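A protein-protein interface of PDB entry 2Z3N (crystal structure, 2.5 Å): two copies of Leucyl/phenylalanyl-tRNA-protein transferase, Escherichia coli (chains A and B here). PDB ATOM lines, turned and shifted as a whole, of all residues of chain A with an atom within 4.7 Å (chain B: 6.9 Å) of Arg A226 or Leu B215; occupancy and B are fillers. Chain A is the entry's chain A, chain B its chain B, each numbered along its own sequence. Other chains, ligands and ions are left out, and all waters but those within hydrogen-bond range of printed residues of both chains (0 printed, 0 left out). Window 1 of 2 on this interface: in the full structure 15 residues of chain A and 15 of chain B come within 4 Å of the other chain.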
ATOM      1  N   VAL A  88      -0.179  14.789   6.639  1.00  0.00           N
ATOM      2  CA  VAL A  88       0.010  15.565   7.860  1.00  0.00           C
ATOM      3  C   VAL A  88      -1.022  16.672   8.011  1.00  0.00           C
ATOM      4  O   VAL A  88      -1.262  17.447   7.082  1.00  0.00           O
ATOM      5  CB  VAL A  88       1.399  16.188   7.915  1.00  0.00           C
ATOM      6  CG1 VAL A  88       1.599  16.868   9.265  1.00  0.00           C
ATOM      7  CG2 VAL A  88       2.450  15.114   7.668  1.00  0.00           C
ATOM      8  N   THR A  89      -1.611  16.744   9.200  1.00  0.00           N
ATOM      9  CA  THR A  89      -2.631  17.733   9.508  1.00  0.00           C
ATOM     10  C   THR A  89      -2.266  18.542  10.751  1.00  0.00           C
ATOM     11  O   THR A  89      -1.313  18.221  11.475  1.00  0.00           O
ATOM     12  CB  THR A  89      -3.984  17.057   9.776  1.00  0.00           C
ATOM     13  OG1 THR A  89      -3.854  16.197  10.918  1.00  0.00           O
ATOM     14  CG2 THR A  89      -4.434  16.216   8.561  1.00  0.00           C
ATOM     15  N   MET A  90      -3.044  19.595  10.991  1.00  0.00           N
ATOM     16  CA  MET A  90      -2.843  20.460  12.140  1.00  0.00           C
ATOM     17  C   MET A  90      -4.140  20.577  12.921  1.00  0.00           C
ATOM     18  O   MET A  90      -5.193  20.844  12.348  1.00  0.00           O
ATOM     19  CB  MET A  90      -2.396  21.856  11.700  1.00  0.00           C
ATOM     20  CG  MET A  90      -2.307  22.844  12.851  1.00  0.00           C
ATOM     21  SD  MET A  90      -1.949  24.499  12.268  1.00  0.00           S
ATOM     22  CE  MET A  90      -0.155  24.393  12.027  1.00  0.00           C
ATOM     23  N   TYR A  92      -6.171  18.473  14.138  1.00  0.00           N
ATOM     24  CA  TYR A  92      -7.233  17.551  13.739  1.00  0.00           C
ATOM     25  C   TYR A  92      -7.616  16.651  14.909  1.00  0.00           C
ATOM     26  O   TYR A  92      -8.787  16.355  15.108  1.00  0.00           O
ATOM     27  CB  TYR A  92      -6.749  16.647  12.605  1.00  0.00           C
ATOM     28  CG  TYR A  92      -7.176  17.029  11.207  1.00  0.00           C
ATOM     29  CD1 TYR A  92      -7.216  18.362  10.796  1.00  0.00           C
ATOM     30  CD2 TYR A  92      -7.471  16.044  10.269  1.00  0.00           C
ATOM     31  CE1 TYR A  92      -7.537  18.694   9.478  1.00  0.00           C
ATOM     32  CE2 TYR A  92      -7.789  16.364   8.960  1.00  0.00           C
ATOM     33  CZ  TYR A  92      -7.819  17.683   8.568  1.00  0.00           C
ATOM     34  OH  TYR A  92      -8.110  17.982   7.258  1.00  0.00           O
ATOM     35  N   GLU A 175       6.072  24.789   7.188  1.00  0.00           N
ATOM     36  CA  GLU A 175       4.891  25.629   7.357  1.00  0.00           C
ATOM     37  C   GLU A 175       5.196  26.797   8.301  1.00  0.00           C
ATOM     38  O   GLU A 175       4.941  27.962   7.985  1.00  0.00           O
ATOM     39  CB  GLU A 175       3.756  24.787   7.941  1.00  0.00           C
ATOM     40  CG  GLU A 175       2.417  25.480   7.939  1.00  0.00           C
ATOM     41  CD  GLU A 175       1.848  25.629   6.543  1.00  0.00           C
ATOM     42  OE1 GLU A 175       0.871  26.381   6.370  1.00  0.00           O
ATOM     43  OE2 GLU A 175       2.377  24.983   5.621  1.00  0.00           O
ATOM     44  N   ASN A 221      -4.991  33.044  11.073  1.00  0.00           N
ATOM     45  CA  ASN A 221      -5.652  31.748  10.953  1.00  0.00           C
ATOM     46  C   ASN A 221      -4.662  30.591  10.869  1.00  0.00           C
ATOM     47  O   ASN A 221      -5.045  29.460  10.551  1.00  0.00           O
ATOM     48  CB  ASN A 221      -6.519  31.755   9.704  1.00  0.00           C
ATOM     49  CG  ASN A 221      -5.692  31.803   8.449  1.00  0.00           C
ATOM     50  OD1 ASN A 221      -4.520  32.196   8.482  1.00  0.00           O
ATOM     51  ND2 ASN A 221      -6.287  31.413   7.328  1.00  0.00           N
ATOM     52  N   PHE A 222      -3.399  30.889  11.156  1.00  0.00           N
ATOM     53  CA  PHE A 222      -2.320  29.906  11.104  1.00  0.00           C
ATOM     54  C   PHE A 222      -2.608  28.582  11.798  1.00  0.00           C
ATOM     55  O   PHE A 222      -2.233  27.529  11.296  1.00  0.00           O
ATOM     56  CB  PHE A 222      -1.039  30.495  11.698  1.00  0.00           C
ATOM     57  CG  PHE A 222       0.141  29.564  11.628  1.00  0.00           C
ATOM     58  CD1 PHE A 222       0.944  29.523  10.492  1.00  0.00           C
ATOM     59  CD2 PHE A 222       0.418  28.693  12.681  1.00  0.00           C
ATOM     60  CE1 PHE A 222       2.003  28.628  10.398  1.00  0.00           C
ATOM     61  CE2 PHE A 222       1.474  27.791  12.599  1.00  0.00           C
ATOM     62  CZ  PHE A 222       2.270  27.757  11.451  1.00  0.00           C
ATOM     63  N   VAL A 224      -5.723  27.264  12.521  1.00  0.00           N
ATOM     64  CA  VAL A 224      -7.024  26.633  12.293  1.00  0.00           C
ATOM     65  C   VAL A 224      -6.735  25.237  11.764  1.00  0.00           C
ATOM     66  O   VAL A 224      -5.721  25.011  11.096  1.00  0.00           O
ATOM     67  CB  VAL A 224      -7.887  27.388  11.259  1.00  0.00           C
ATOM     68  CG1 VAL A 224      -7.931  28.868  11.603  1.00  0.00           C
ATOM     69  CG2 VAL A 224      -7.355  27.154   9.851  1.00  0.00           C
ATOM     70  N   PRO A 225      -7.607  24.275  12.077  1.00  0.00           N
ATOM     71  CA  PRO A 225      -7.370  22.910  11.593  1.00  0.00           C
ATOM     72  C   PRO A 225      -7.365  22.788  10.073  1.00  0.00           C
ATOM     73  O   PRO A 225      -8.314  23.202   9.411  1.00  0.00           O
ATOM     74  CB  PRO A 225      -8.482  22.094  12.268  1.00  0.00           C
ATOM     75  CG  PRO A 225      -9.500  23.130  12.718  1.00  0.00           C
ATOM     76  CD  PRO A 225      -8.679  24.319  13.087  1.00  0.00           C
ATOM     77  N   ARG A 226      -6.292  22.216   9.527  1.00  0.00           N
ATOM     78  CA  ARG A 226      -6.168  22.050   8.086  1.00  0.00           C
ATOM     79  C   ARG A 226      -5.159  20.971   7.683  1.00  0.00           C
ATOM     80  O   ARG A 226      -4.310  20.567   8.477  1.00  0.00           O
ATOM     81  CB  ARG A 226      -5.753  23.379   7.450  1.00  0.00           C
ATOM     82  CG  ARG A 226      -4.415  23.914   7.947  1.00  0.00           C
ATOM     83  CD  ARG A 226      -4.550  25.369   8.392  1.00  0.00           C
ATOM     84  NE  ARG A 226      -3.355  25.882   9.062  1.00  0.00           N
ATOM     85  CZ  ARG A 226      -2.219  26.171   8.439  1.00  0.00           C
ATOM     86  NH1 ARG A 226      -2.119  26.004   7.123  1.00  0.00           N
ATOM     87  NH2 ARG A 226      -1.178  26.619   9.131  1.00  0.00           N
ATOM     88  N   CYS A 227      -5.258  20.503   6.443  1.00  0.00           N
ATOM     89  CA  CYS A 227      -4.326  19.506   5.941  1.00  0.00           C
ATOM     90  C   CYS A 227      -3.106  20.342   5.580  1.00  0.00           C
ATOM     91  O   CYS A 227      -3.251  21.454   5.075  1.00  0.00           O
ATOM     92  CB  CYS A 227      -4.896  18.816   4.692  1.00  0.00           C
ATOM     93  SG  CYS A 227      -4.139  17.214   4.244  1.00  0.00           S
ATOM     94  N   LEU A 228      -1.910  19.829   5.873  1.00  0.00           N
ATOM     95  CA  LEU A 228      -0.670  20.543   5.564  1.00  0.00           C
ATOM     96  C   LEU A 228       0.139  19.829   4.487  1.00  0.00           C
ATOM     97  O   LEU A 228       0.956  20.441   3.806  1.00  0.00           O
ATOM     98  CB  LEU A 228       0.221  20.661   6.806  1.00  0.00           C
ATOM     99  CG  LEU A 228      -0.248  21.367   8.080  1.00  0.00           C
ATOM    100  CD1 LEU A 228       0.836  21.202   9.153  1.00  0.00           C
ATOM    101  CD2 LEU A 228      -0.529  22.842   7.812  1.00  0.00           C
ATOM    102  N   GLN B  42     -14.261  18.145   4.415  1.00  0.00           N
ATOM    103  CA  GLN B  42     -13.341  19.106   3.834  1.00  0.00           C
ATOM    104  C   GLN B  42     -13.524  19.143   2.310  1.00  0.00           C
ATOM    105  O   GLN B  42     -13.162  20.126   1.648  1.00  0.00           O
ATOM    106  CB  GLN B  42     -11.920  18.680   4.191  1.00  0.00           C
ATOM    107  CG  GLN B  42     -10.806  19.492   3.574  1.00  0.00           C
ATOM    108  CD  GLN B  42      -9.448  18.898   3.898  1.00  0.00           C
ATOM    109  OE1 GLN B  42      -8.403  19.446   3.527  1.00  0.00           O
ATOM    110  NE2 GLN B  42      -9.459  17.768   4.600  1.00  0.00           N
ATOM    111  N   GLN B 148     -16.559  23.850  10.222  1.00  0.00           N
ATOM    112  CA  GLN B 148     -15.658  23.860   9.084  1.00  0.00           C
ATOM    113  C   GLN B 148     -15.281  25.339   8.936  1.00  0.00           C
ATOM    114  O   GLN B 148     -15.675  26.020   7.975  1.00  0.00           O
ATOM    115  CB  GLN B 148     -16.414  23.357   7.848  1.00  0.00           C
ATOM    116  CG  GLN B 148     -15.598  22.628   6.792  1.00  0.00           C
ATOM    117  CD  GLN B 148     -14.940  21.354   7.306  1.00  0.00           C
ATOM    118  OE1 GLN B 148     -15.418  20.731   8.256  1.00  0.00           O
ATOM    119  NE2 GLN B 148     -13.846  20.957   6.672  1.00  0.00           N
ATOM    120  N   GLY B 149     -14.516  25.835   9.904  1.00  0.00           N
ATOM    121  CA  GLY B 149     -14.130  27.229   9.872  1.00  0.00           C
ATOM    122  C   GLY B 149     -15.345  28.067  10.222  1.00  0.00           C
ATOM    123  O   GLY B 149     -15.964  27.849  11.273  1.00  0.00           O
ATOM    124  N   THR B 150     -15.694  29.004   9.341  1.00  0.00           N
ATOM    125  CA  THR B 150     -16.836  29.896   9.543  1.00  0.00           C
ATOM    126  C   THR B 150     -18.103  29.301   8.931  1.00  0.00           C
ATOM    127  O   THR B 150     -19.147  29.960   8.823  1.00  0.00           O
ATOM    128  CB  THR B 150     -16.578  31.255   8.891  1.00  0.00           C
ATOM    129  OG1 THR B 150     -16.275  31.052   7.509  1.00  0.00           O
ATOM    130  CG2 THR B 150     -15.402  31.972   9.567  1.00  0.00           C
ATOM    131  N   LEU B 210     -17.216  26.596   0.754  1.00  0.00           N
ATOM    132  CA  LEU B 210     -16.560  25.658   1.659  1.00  0.00           C
ATOM    133  C   LEU B 210     -15.036  25.826   1.686  1.00  0.00           C
ATOM    134  O   LEU B 210     -14.433  25.839   2.760  1.00  0.00           O
ATOM    135  CB  LEU B 210     -16.948  24.222   1.268  1.00  0.00           C
ATOM    136  CG  LEU B 210     -16.360  22.967   1.932  1.00  0.00           C
ATOM    137  CD1 LEU B 210     -14.955  22.733   1.407  1.00  0.00           C
ATOM    138  CD2 LEU B 210     -16.369  23.099   3.444  1.00  0.00           C
ATOM    139  N   ASN B 211     -14.414  25.957   0.515  1.00  0.00           N
ATOM    140  CA  ASN B 211     -12.962  26.136   0.447  1.00  0.00           C
ATOM    141  C   ASN B 211     -12.562  27.479   1.062  1.00  0.00           C
ATOM    142  O   ASN B 211     -11.469  27.635   1.594  1.00  0.00           O
ATOM    143  CB  ASN B 211     -12.468  26.093  -1.006  1.00  0.00           C
ATOM    144  CG  ASN B 211     -10.944  26.231  -1.114  1.00  0.00           C
ATOM    145  OD1 ASN B 211     -10.410  26.614  -2.158  1.00  0.00           O
ATOM    146  ND2 ASN B 211     -10.241  25.909  -0.029  1.00  0.00           N
ATOM    147  N   GLN B 212     -13.471  28.441   0.981  1.00  0.00           N
ATOM    148  CA  GLN B 212     -13.259  29.783   1.508  1.00  0.00           C
ATOM    149  C   GLN B 212     -13.436  29.807   3.035  1.00  0.00           C
ATOM    150  O   GLN B 212     -12.615  30.353   3.770  1.00  0.00           O
ATOM    151  CB  GLN B 212     -14.277  30.730   0.861  1.00  0.00           C
ATOM    152  CG  GLN B 212     -13.726  32.053   0.355  1.00  0.00           C
ATOM    153  CD  GLN B 212     -12.850  31.893  -0.861  1.00  0.00           C
ATOM    154  OE1 GLN B 212     -11.704  31.458  -0.762  1.00  0.00           O
ATOM    155  NE2 GLN B 212     -13.388  32.235  -2.027  1.00  0.00           N
ATOM    156  N   MET B 213     -14.512  29.194   3.509  1.00  0.00           N
ATOM    157  CA  MET B 213     -14.812  29.186   4.927  1.00  0.00           C
ATOM    158  C   MET B 213     -14.053  28.191   5.795  1.00  0.00           C
ATOM    159  O   MET B 213     -13.884  28.429   6.990  1.00  0.00           O
ATOM    160  CB  MET B 213     -16.314  28.999   5.109  1.00  0.00           C
ATOM    161  CG  MET B 213     -17.099  30.207   4.679  1.00  0.00           C
ATOM    162  SD  MET B 213     -18.807  29.839   4.290  1.00  0.00           S
ATOM    163  CE  MET B 213     -19.100  31.017   2.968  1.00  0.00           C
ATOM    164  N   ARG B 214     -13.588  27.086   5.221  1.00  0.00           N
ATOM    165  CA  ARG B 214     -12.868  26.110   6.038  1.00  0.00           C
ATOM    166  C   ARG B 214     -11.610  26.673   6.686  1.00  0.00           C
ATOM    167  O   ARG B 214     -11.177  26.174   7.721  1.00  0.00           O
ATOM    168  CB  ARG B 214     -12.525  24.837   5.235  1.00  0.00           C
ATOM    169  CG  ARG B 214     -11.842  25.039   3.886  1.00  0.00           C
ATOM    170  CD  ARG B 214     -11.575  23.684   3.205  1.00  0.00           C
ATOM    171  NE  ARG B 214     -10.291  23.126   3.616  1.00  0.00           N
ATOM    172  CZ  ARG B 214      -9.124  23.503   3.104  1.00  0.00           C
ATOM    173  NH1 ARG B 214      -9.085  24.428   2.153  1.00  0.00           N
ATOM    174  NH2 ARG B 214      -7.990  22.987   3.565  1.00  0.00           N
ATOM    175  N   LEU B 215     -11.035  27.720   6.103  1.00  0.00           N
ATOM    176  CA  LEU B 215      -9.816  28.295   6.663  1.00  0.00           C
ATOM    177  C   LEU B 215     -10.008  29.578   7.466  1.00  0.00           C
ATOM    178  O   LEU B 215      -9.040  30.173   7.935  1.00  0.00           O
ATOM    179  CB  LEU B 215      -8.776  28.518   5.560  1.00  0.00           C
ATOM    180  CG  LEU B 215      -8.258  27.237   4.901  1.00  0.00           C
ATOM    181  CD1 LEU B 215      -7.159  27.591   3.905  1.00  0.00           C
ATOM    182  CD2 LEU B 215      -7.733  26.269   5.966  1.00  0.00           C
ATOM    183  N   GLY B 216     -11.256  30.007   7.615  1.00  0.00           N
ATOM    184  CA  GLY B 216     -11.527  31.190   8.405  1.00  0.00           C
ATOM    185  C   GLY B 216     -11.637  30.705   9.837  1.00  0.00           C
ATOM    186  O   GLY B 216     -11.595  29.501  10.080  1.00  0.00           O
ATOM    187  N   ARG B 217     -11.766  31.615  10.792  1.00  0.00           N
ATOM    188  CA  ARG B 217     -11.891  31.197  12.183  1.00  0.00           C
ATOM    189  C   ARG B 217     -12.790  32.098  13.019  1.00  0.00           C
ATOM    190  O   ARG B 217     -13.033  33.255  12.674  1.00  0.00           O
ATOM    191  CB  ARG B 217     -10.509  31.095  12.852  1.00  0.00           C
ATOM    192  CG  ARG B 217      -9.620  32.323  12.717  1.00  0.00           C
ATOM    193  CD  ARG B 217      -8.511  32.330  13.778  1.00  0.00           C
ATOM    194  NE  ARG B 217      -9.028  32.739  15.084  1.00  0.00           N
ATOM    195  CZ  ARG B 217      -8.331  32.738  16.218  1.00  0.00           C
ATOM    196  NH1 ARG B 217      -7.063  32.348  16.225  1.00  0.00           N
ATOM    197  NH2 ARG B 217      -8.915  33.111  17.351  1.00  0.00           N
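NE2 of Gln B42 lies within hydrogen-bond range of OH of Tyr A92, at 3.0 Å.
The side-chain amide nitrogen (ND2) of Asn A221 lies within hydrogen-bond range of the backbone carbonyl oxygen (O) of Leu B215 (3.1 Å).
Leu B215 touches just these residues of chain A: Asn A221 (3.1 Å), Val A224 (3.95 Å) and Arg A226 (3.8 Å).
Of the printed residues of chain B, Tyr A92 touches Gln B42.
Of the printed residues of chain B, Cys A227 touches Gln B42.
Of the printed residues of chain A, Gln B42 touches Tyr A92 (3.0 Å) and Cys A227 (3.7 Å).
Of the printed residues of chain B, Val A224 touches Leu B215 and Arg B217.
Of the printed residues of chain A, Arg B217 touches Val A224.
Val A88 touches none of the printed residues of chain B.
The nearest residue of chain A that does not touch Leu B215 is Pro A225 (4.6 Å).
Printed residues of chain B that touch a printed residue of chain A: Gln B42, Leu B215 and Arg B217.
Of the 12 printed residues of chain A, 5 touch a printed residue of chain B.
Hydrophobic or aromatic side chains of chain A within 4 Å of the printed part of chain B: Tyr A92 and Val A224.
Among the printed residues, no Asp or Glu carboxylate lies within 4 Å of a Lys or Arg side-chain nitrogen of the other chain.
N of Met A90 is in hydrogen-bond range of O of Arg A226, 3.0 Å away.
The side-chain carboxylate (OE1) of Glu A175 is in salt-bridge range of the guanidinium group (NH1) of Arg A226, at 3.1 Å.
O of Phe A222 is in hydrogen-bond range of NH2 of Arg A226 (2.6 Å).
The backbone carbonyl oxygen (O) of Val A224 sits close to the guanidinium group (NE) of Arg A226, 3.2 Å away.
No position is printed for both chains.
Val A224 touches Leu B215.
Val A224 touches Arg B217 (CG1 to CB, 3.6 Å).
Arg A226 touches Leu B215 (CB to CD2, 3.8 Å).
Cys A227 touches Gln B42.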
